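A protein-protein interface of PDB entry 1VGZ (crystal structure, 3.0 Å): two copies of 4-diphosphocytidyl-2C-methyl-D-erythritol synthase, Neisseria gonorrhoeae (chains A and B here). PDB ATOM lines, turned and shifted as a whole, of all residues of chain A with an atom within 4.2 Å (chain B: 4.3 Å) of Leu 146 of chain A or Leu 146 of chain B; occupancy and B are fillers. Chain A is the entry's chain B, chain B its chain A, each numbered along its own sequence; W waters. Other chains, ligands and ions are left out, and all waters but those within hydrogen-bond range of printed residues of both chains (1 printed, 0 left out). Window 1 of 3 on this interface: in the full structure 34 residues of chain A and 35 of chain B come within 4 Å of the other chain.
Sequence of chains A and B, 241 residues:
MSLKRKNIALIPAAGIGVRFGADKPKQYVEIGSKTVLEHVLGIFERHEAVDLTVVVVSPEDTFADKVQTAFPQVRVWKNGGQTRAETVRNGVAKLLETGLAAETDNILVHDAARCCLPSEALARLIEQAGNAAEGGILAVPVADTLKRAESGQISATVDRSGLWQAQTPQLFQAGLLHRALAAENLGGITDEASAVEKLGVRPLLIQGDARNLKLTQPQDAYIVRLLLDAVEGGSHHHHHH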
ATOM      1  N   VAL A 142     -15.334   2.582 -27.485  1.00  0.00           N
ATOM      2  CA  VAL A 142     -14.421   3.224 -28.446  1.00  0.00           C
ATOM      3  C   VAL A 142     -14.547   2.507 -29.792  1.00  0.00           C
ATOM      4  O   VAL A 142     -14.350   1.295 -29.877  1.00  0.00           O
ATOM      5  CB  VAL A 142     -12.964   3.215 -27.982  1.00  0.00           C
ATOM      6  CG1 VAL A 142     -12.066   3.778 -29.083  1.00  0.00           C
ATOM      7  CG2 VAL A 142     -12.790   4.043 -26.718  1.00  0.00           C
ATOM      8  N   ASP A 144     -13.218   3.731 -33.106  1.00  0.00           N
ATOM      9  CA  ASP A 144     -12.017   4.065 -33.773  1.00  0.00           C
ATOM     10  C   ASP A 144     -10.688   3.608 -33.211  1.00  0.00           C
ATOM     11  O   ASP A 144     -10.456   3.610 -32.011  1.00  0.00           O
ATOM     12  CB  ASP A 144     -11.943   5.634 -33.826  1.00  0.00           C
ATOM     13  CG  ASP A 144     -13.130   6.129 -34.638  1.00  0.00           C
ATOM     14  OD1 ASP A 144     -13.507   7.312 -34.538  1.00  0.00           O
ATOM     15  OD2 ASP A 144     -13.693   5.286 -35.379  1.00  0.00           O
ATOM     16  N   THR A 145      -9.740   3.343 -34.132  1.00  0.00           N
ATOM     17  CA  THR A 145      -8.393   2.946 -33.734  1.00  0.00           C
ATOM     18  C   THR A 145      -7.818   4.086 -32.896  1.00  0.00           C
ATOM     19  O   THR A 145      -8.095   5.241 -33.232  1.00  0.00           O
ATOM     20  CB  THR A 145      -7.503   2.691 -34.956  1.00  0.00           C
ATOM     21  OG1 THR A 145      -8.015   1.555 -35.664  1.00  0.00           O
ATOM     22  CG2 THR A 145      -6.065   2.361 -34.576  1.00  0.00           C
ATOM     23  N   LEU A 146      -7.079   3.759 -31.842  1.00  0.00           N
ATOM     24  CA  LEU A 146      -6.507   4.823 -31.001  1.00  0.00           C
ATOM     25  C   LEU A 146      -5.026   5.016 -31.285  1.00  0.00           C
ATOM     26  O   LEU A 146      -4.270   4.036 -31.257  1.00  0.00           O
ATOM     27  CB  LEU A 146      -6.677   4.490 -29.524  1.00  0.00           C
ATOM     28  CG  LEU A 146      -7.765   5.105 -28.673  1.00  0.00           C
ATOM     29  CD1 LEU A 146      -7.192   5.392 -27.277  1.00  0.00           C
ATOM     30  CD2 LEU A 146      -8.349   6.392 -29.234  1.00  0.00           C
ATOM     31  N   LYS A 147      -4.556   6.254 -31.337  1.00  0.00           N
ATOM     32  CA  LYS A 147      -3.163   6.512 -31.631  1.00  0.00           C
ATOM     33  C   LYS A 147      -2.474   7.437 -30.642  1.00  0.00           C
ATOM     34  O   LYS A 147      -2.915   8.562 -30.403  1.00  0.00           O
ATOM     35  CB  LYS A 147      -2.995   7.173 -33.020  1.00  0.00           C
ATOM     36  CG  LYS A 147      -3.570   6.498 -34.217  1.00  0.00           C
ATOM     37  CD  LYS A 147      -2.939   5.176 -34.619  1.00  0.00           C
ATOM     38  CE  LYS A 147      -3.448   4.767 -35.999  1.00  0.00           C
ATOM     39  NZ  LYS A 147      -3.312   3.320 -36.296  1.00  0.00           N
ATOM     40  N   THR A 157       0.183   2.862 -31.622  1.00  0.00           N
ATOM     41  CA  THR A 157      -1.222   2.510 -31.665  1.00  0.00           C
ATOM     42  C   THR A 157      -1.555   1.821 -30.323  1.00  0.00           C
ATOM     43  O   THR A 157      -0.746   1.006 -29.871  1.00  0.00           O
ATOM     44  CB  THR A 157      -1.594   1.504 -32.766  1.00  0.00           C
ATOM     45  OG1 THR A 157      -2.953   1.069 -32.543  1.00  0.00           O
ATOM     46  CG2 THR A 157      -0.731   0.250 -32.702  1.00  0.00           C
ATOM     47  N   VAL A 158      -2.614   2.265 -29.657  1.00  0.00           N
ATOM     48  CA  VAL A 158      -2.981   1.639 -28.378  1.00  0.00           C
ATOM     49  C   VAL A 158      -4.197   0.747 -28.589  1.00  0.00           C
ATOM     50  O   VAL A 158      -5.100   1.067 -29.366  1.00  0.00           O
ATOM     51  CB  VAL A 158      -3.193   2.656 -27.266  1.00  0.00           C
ATOM     52  CG1 VAL A 158      -2.058   3.666 -27.214  1.00  0.00           C
ATOM     53  CG2 VAL A 158      -4.515   3.382 -27.398  1.00  0.00           C
ATOM     54  N   LEU A 163     -12.508  -0.862 -24.496  1.00  0.00           N
ATOM     55  CA  LEU A 163     -12.382   0.484 -23.974  1.00  0.00           C
ATOM     56  C   LEU A 163     -13.650   1.282 -24.297  1.00  0.00           C
ATOM     57  O   LEU A 163     -14.332   0.998 -25.284  1.00  0.00           O
ATOM     58  CB  LEU A 163     -11.197   1.215 -24.572  1.00  0.00           C
ATOM     59  CG  LEU A 163      -9.791   0.891 -24.124  1.00  0.00           C
ATOM     60  CD1 LEU A 163      -8.849   2.015 -24.561  1.00  0.00           C
ATOM     61  CD2 LEU A 163      -9.711   0.714 -22.616  1.00  0.00           C
ATOM     62  N   TRP A 164     -14.026   2.155 -23.361  1.00  0.00           N
ATOM     63  CA  TRP A 164     -15.210   2.985 -23.473  1.00  0.00           C
ATOM     64  C   TRP A 164     -14.886   4.454 -23.214  1.00  0.00           C
ATOM     65  O   TRP A 164     -13.978   4.760 -22.445  1.00  0.00           O
ATOM     66  CB  TRP A 164     -16.296   2.577 -22.477  1.00  0.00           C
ATOM     67  CG  TRP A 164     -16.902   1.238 -22.739  1.00  0.00           C
ATOM     68  CD1 TRP A 164     -16.285   0.030 -22.580  1.00  0.00           C
ATOM     69  CD2 TRP A 164     -18.227   0.941 -23.174  1.00  0.00           C
ATOM     70  NE1 TRP A 164     -17.124  -0.991 -22.931  1.00  0.00           N
ATOM     71  CE2 TRP A 164     -18.334  -0.460 -23.286  1.00  0.00           C
ATOM     72  CE3 TRP A 164     -19.361   1.703 -23.449  1.00  0.00           C
ATOM     73  CZ2 TRP A 164     -19.508  -1.095 -23.693  1.00  0.00           C
ATOM     74  CZ3 TRP A 164     -20.525   1.086 -23.866  1.00  0.00           C
ATOM     75  CH2 TRP A 164     -20.587  -0.307 -23.982  1.00  0.00           C
ATOM     76  N   GLN A 165     -15.598   5.333 -23.909  1.00  0.00           N
ATOM     77  CA  GLN A 165     -15.410   6.769 -23.703  1.00  0.00           C
ATOM     78  C   GLN A 165     -16.446   7.200 -22.648  1.00  0.00           C
ATOM     79  O   GLN A 165     -17.645   6.980 -22.861  1.00  0.00           O
ATOM     80  CB  GLN A 165     -15.610   7.545 -24.995  1.00  0.00           C
ATOM     81  CG  GLN A 165     -14.816   7.062 -26.186  1.00  0.00           C
ATOM     82  CD  GLN A 165     -14.895   7.959 -27.410  1.00  0.00           C
ATOM     83  OE1 GLN A 165     -15.417   7.568 -28.464  1.00  0.00           O
ATOM     84  NE2 GLN A 165     -14.371   9.181 -27.271  1.00  0.00           N
ATOM     85  N   VAL B 142      -8.536  12.634 -28.263  1.00  0.00           N
ATOM     86  CA  VAL B 142      -9.501  12.039 -27.332  1.00  0.00           C
ATOM     87  C   VAL B 142      -9.902  13.089 -26.291  1.00  0.00           C
ATOM     88  O   VAL B 142      -9.064  13.564 -25.524  1.00  0.00           O
ATOM     89  CB  VAL B 142      -8.934  10.813 -26.606  1.00  0.00           C
ATOM     90  CG1 VAL B 142      -9.996  10.229 -25.674  1.00  0.00           C
ATOM     91  CG2 VAL B 142      -8.487   9.753 -27.590  1.00  0.00           C
ATOM     92  N   ASP B 144     -12.790  12.896 -23.971  1.00  0.00           N
ATOM     93  CA  ASP B 144     -13.308  12.084 -22.940  1.00  0.00           C
ATOM     94  C   ASP B 144     -12.431  11.093 -22.205  1.00  0.00           C
ATOM     95  O   ASP B 144     -11.824  10.220 -22.812  1.00  0.00           O
ATOM     96  CB  ASP B 144     -14.443  11.223 -23.613  1.00  0.00           C
ATOM     97  CG  ASP B 144     -15.502  12.179 -24.148  1.00  0.00           C
ATOM     98  OD1 ASP B 144     -16.367  11.757 -24.945  1.00  0.00           O
ATOM     99  OD2 ASP B 144     -15.456  13.368 -23.758  1.00  0.00           O
ATOM    100  N   THR B 145     -12.617  11.015 -20.879  1.00  0.00           N
ATOM    101  CA  THR B 145     -11.905  10.065 -20.030  1.00  0.00           C
ATOM    102  C   THR B 145     -12.166   8.680 -20.618  1.00  0.00           C
ATOM    103  O   THR B 145     -13.291   8.408 -21.040  1.00  0.00           O
ATOM    104  CB  THR B 145     -12.376  10.111 -18.568  1.00  0.00           C
ATOM    105  OG1 THR B 145     -11.977  11.352 -17.967  1.00  0.00           O
ATOM    106  CG2 THR B 145     -11.750   9.030 -17.690  1.00  0.00           C
ATOM    107  N   LEU B 146     -11.125   7.863 -20.687  1.00  0.00           N
ATOM    108  CA  LEU B 146     -11.273   6.513 -21.242  1.00  0.00           C
ATOM    109  C   LEU B 146     -11.363   5.488 -20.114  1.00  0.00           C
ATOM    110  O   LEU B 146     -10.583   5.575 -19.163  1.00  0.00           O
ATOM    111  CB  LEU B 146     -10.081   6.128 -22.111  1.00  0.00           C
ATOM    112  CG  LEU B 146      -9.900   6.633 -23.525  1.00  0.00           C
ATOM    113  CD1 LEU B 146      -8.981   5.650 -24.264  1.00  0.00           C
ATOM    114  CD2 LEU B 146     -11.191   6.804 -24.299  1.00  0.00           C
ATOM    115  N   LYS B 147     -12.230   4.496 -20.252  1.00  0.00           N
ATOM    116  CA  LYS B 147     -12.373   3.495 -19.218  1.00  0.00           C
ATOM    117  C   LYS B 147     -12.278   2.080 -19.767  1.00  0.00           C
ATOM    118  O   LYS B 147     -12.942   1.743 -20.741  1.00  0.00           O
ATOM    119  CB  LYS B 147     -13.749   3.606 -18.524  1.00  0.00           C
ATOM    120  CG  LYS B 147     -14.135   4.948 -17.973  1.00  0.00           C
ATOM    121  CD  LYS B 147     -13.410   5.311 -16.681  1.00  0.00           C
ATOM    122  CE  LYS B 147     -13.904   6.661 -16.174  1.00  0.00           C
ATOM    123  NZ  LYS B 147     -13.089   7.202 -15.060  1.00  0.00           N
ATOM    124  N   THR B 157      -9.290   2.924 -15.477  1.00  0.00           N
ATOM    125  CA  THR B 157      -9.304   4.160 -16.248  1.00  0.00           C
ATOM    126  C   THR B 157      -7.937   4.232 -16.962  1.00  0.00           C
ATOM    127  O   THR B 157      -6.924   3.955 -16.307  1.00  0.00           O
ATOM    128  CB  THR B 157      -9.467   5.432 -15.412  1.00  0.00           C
ATOM    129  OG1 THR B 157      -9.185   6.596 -16.220  1.00  0.00           O
ATOM    130  CG2 THR B 157      -8.475   5.462 -14.252  1.00  0.00           C
ATOM    131  N   VAL B 158      -7.942   4.456 -18.270  1.00  0.00           N
ATOM    132  CA  VAL B 158      -6.686   4.534 -19.014  1.00  0.00           C
ATOM    133  C   VAL B 158      -6.346   5.984 -19.322  1.00  0.00           C
ATOM    134  O   VAL B 158      -7.200   6.822 -19.608  1.00  0.00           O
ATOM    135  CB  VAL B 158      -6.679   3.662 -20.266  1.00  0.00           C
ATOM    136  CG1 VAL B 158      -7.339   2.315 -19.991  1.00  0.00           C
ATOM    137  CG2 VAL B 158      -7.339   4.327 -21.462  1.00  0.00           C
ATOM    138  N   LEU B 163      -3.565  11.100 -26.647  1.00  0.00           N
ATOM    139  CA  LEU B 163      -4.180  10.079 -27.481  1.00  0.00           C
ATOM    140  C   LEU B 163      -5.142  10.741 -28.470  1.00  0.00           C
ATOM    141  O   LEU B 163      -5.621  11.849 -28.231  1.00  0.00           O
ATOM    142  CB  LEU B 163      -4.926   9.034 -26.689  1.00  0.00           C
ATOM    143  CG  LEU B 163      -4.174   8.091 -25.770  1.00  0.00           C
ATOM    144  CD1 LEU B 163      -5.151   7.051 -25.215  1.00  0.00           C
ATOM    145  CD2 LEU B 163      -3.013   7.414 -26.476  1.00  0.00           C
ATOM    146  N   TRP B 164      -5.235  10.138 -29.648  1.00  0.00           N
ATOM    147  CA  TRP B 164      -6.060  10.622 -30.737  1.00  0.00           C
ATOM    148  C   TRP B 164      -6.932   9.500 -31.291  1.00  0.00           C
ATOM    149  O   TRP B 164      -6.585   8.322 -31.188  1.00  0.00           O
ATOM    150  CB  TRP B 164      -5.192  11.147 -31.891  1.00  0.00           C
ATOM    151  CG  TRP B 164      -4.459  12.405 -31.570  1.00  0.00           C
ATOM    152  CD1 TRP B 164      -3.373  12.529 -30.748  1.00  0.00           C
ATOM    153  CD2 TRP B 164      -4.724  13.721 -32.054  1.00  0.00           C
ATOM    154  NE1 TRP B 164      -2.973  13.835 -30.669  1.00  0.00           N
ATOM    155  CE2 TRP B 164      -3.778  14.592 -31.473  1.00  0.00           C
ATOM    156  CE3 TRP B 164      -5.644  14.258 -32.951  1.00  0.00           C
ATOM    157  CZ2 TRP B 164      -3.749  15.958 -31.739  1.00  0.00           C
ATOM    158  CZ3 TRP B 164      -5.633  15.616 -33.209  1.00  0.00           C
ATOM    159  CH2 TRP B 164      -4.686  16.452 -32.603  1.00  0.00           C
ATOM    160  N   GLN B 165      -8.091   9.871 -31.816  1.00  0.00           N
ATOM    161  CA  GLN B 165      -8.970   8.871 -32.423  1.00  0.00           C
ATOM    162  C   GLN B 165      -8.742   8.937 -33.943  1.00  0.00           C
ATOM    163  O   GLN B 165      -8.839  10.009 -34.547  1.00  0.00           O
ATOM    164  CB  GLN B 165     -10.423   9.083 -32.058  1.00  0.00           C
ATOM    165  CG  GLN B 165     -10.726   9.093 -30.575  1.00  0.00           C
ATOM    166  CD  GLN B 165     -12.174   9.403 -30.244  1.00  0.00           C
ATOM    167  OE1 GLN B 165     -12.540  10.545 -29.935  1.00  0.00           O
ATOM    168  NE2 GLN B 165     -13.025   8.378 -30.311  1.00  0.00           N
HETATM  169  O   HOH W   1     -14.510   6.214 -31.336  1.00  0.00           O
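O of Trp 164 of chain A lies within hydrogen-bond range of N of Lys 147 of chain B, 2.8 Å away.
The backbone carbonyl oxygen (O) of Trp 164 of chain B sits at hydrogen-bond distance from the backbone NH (N) of Lys 147 of chain A.
NE2 of Gln 165 of chain B lies within hydrogen-bond range of OE1 of Gln 165 of chain A (3.1 Å).
The backbone NH (N) of Val 142 of chain B sits at hydrogen-bond distance from the backbone carbonyl oxygen (O) of Leu 163 of chain B (3.0 Å).
OG1 of Thr 157 of chain B sits at hydrogen-bond distance from O of Leu 146 of chain B.
O of Leu 146 of chain B lies within hydrogen-bond range of N of Val 158 of chain B (3.0 Å).
The backbone NH (N) of Val 142 of chain A is in hydrogen-bond range of the backbone carbonyl oxygen (O) of Leu 163 of chain A, at 2.9 Å.
The side-chain hydroxyl (OG1) of Thr 157 of chain A sits close to the backbone carbonyl oxygen (O) of Leu 146 of chain A.
The backbone carbonyl oxygen (O) of Leu 146 of chain A is in hydrogen-bond range of the backbone NH (N) of Val 158 of chain A.
Thr 145 of chain A touches Trp 164 of chain B.
Leu 146 of chain A touches Val 142 of chain B (CD2 to CG2, 3.7 Å).
Leu 146 of chain A touches Leu 163 of chain B (CD1 to CD1, 3.3 Å).
Trp 164 of chain B touches Leu 146 of chain A.
Val 158 of chain A touches Leu 163 of chain B (CG1 to CD2, 3.9 Å).
CD1 of Leu 163 of chain A touches CD1 of Leu 146 of chain B (3.6 Å).
Leu 163 of chain A touches Lys 147 of chain B.
Val 158 of chain B touches Leu 163 of chain A (CG1 to CD2, 3.9 Å).
Leu 146 of chain B touches Trp 164 of chain A.
Gln 165 of chain A touches Thr 145 of chain B (C to O, 3.7 Å).
Printed residues of chain A within 4 Å of Leu 146 of chain B: Leu 146, Leu 163 and Trp 164.
Of the printed residues of chain A, Lys 147 of chain B touches Leu 163 and Trp 164.
Of the printed residues of chain B, Lys 147 of chain A touches Leu 163 and Trp 164.
The nearest printed residue of chain A that does not touch Leu 146 of chain B is Val 142 of chain A (4.004 Å).
Hydrophobic or aromatic side chains of chain A that line the printed part of chain B: Leu 146, Val 158, Leu 163 and Trp 164.
Among the printed residues, no Asp or Glu carboxylate lies within 4 Å of a Lys or Arg side-chain nitrogen of the other chain.
Thr 145 of chain A touches Gln 165 of chain B, and with the chains exchanged Gln 165 of chain A touches Thr 145 of chain B.
Leu 146 of chain B touches its own counterpart, Leu 146 of chain A.
Lys 147 of chain A touches Leu 163 of chain B, and with the chains exchanged Leu 163 of chain A touches Lys 147 of chain B.
Lys 147 of chain A touches Trp 164 of chain B, and with the chains exchanged Trp 164 of chain A touches Lys 147 of chain B.
10 positions are printed for both chains.
Of the 18 pairs that touch across the chains among the printed residues, 16 have their exchanged pair printed and touching as well.
Water W1 lies within hydrogen-bond range of the side-chain amide nitrogen of Gln 165 of chain B, the side-chain amide oxygen of Gln 165 of chain A and the backbone NH of Asp 144 of chain A.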
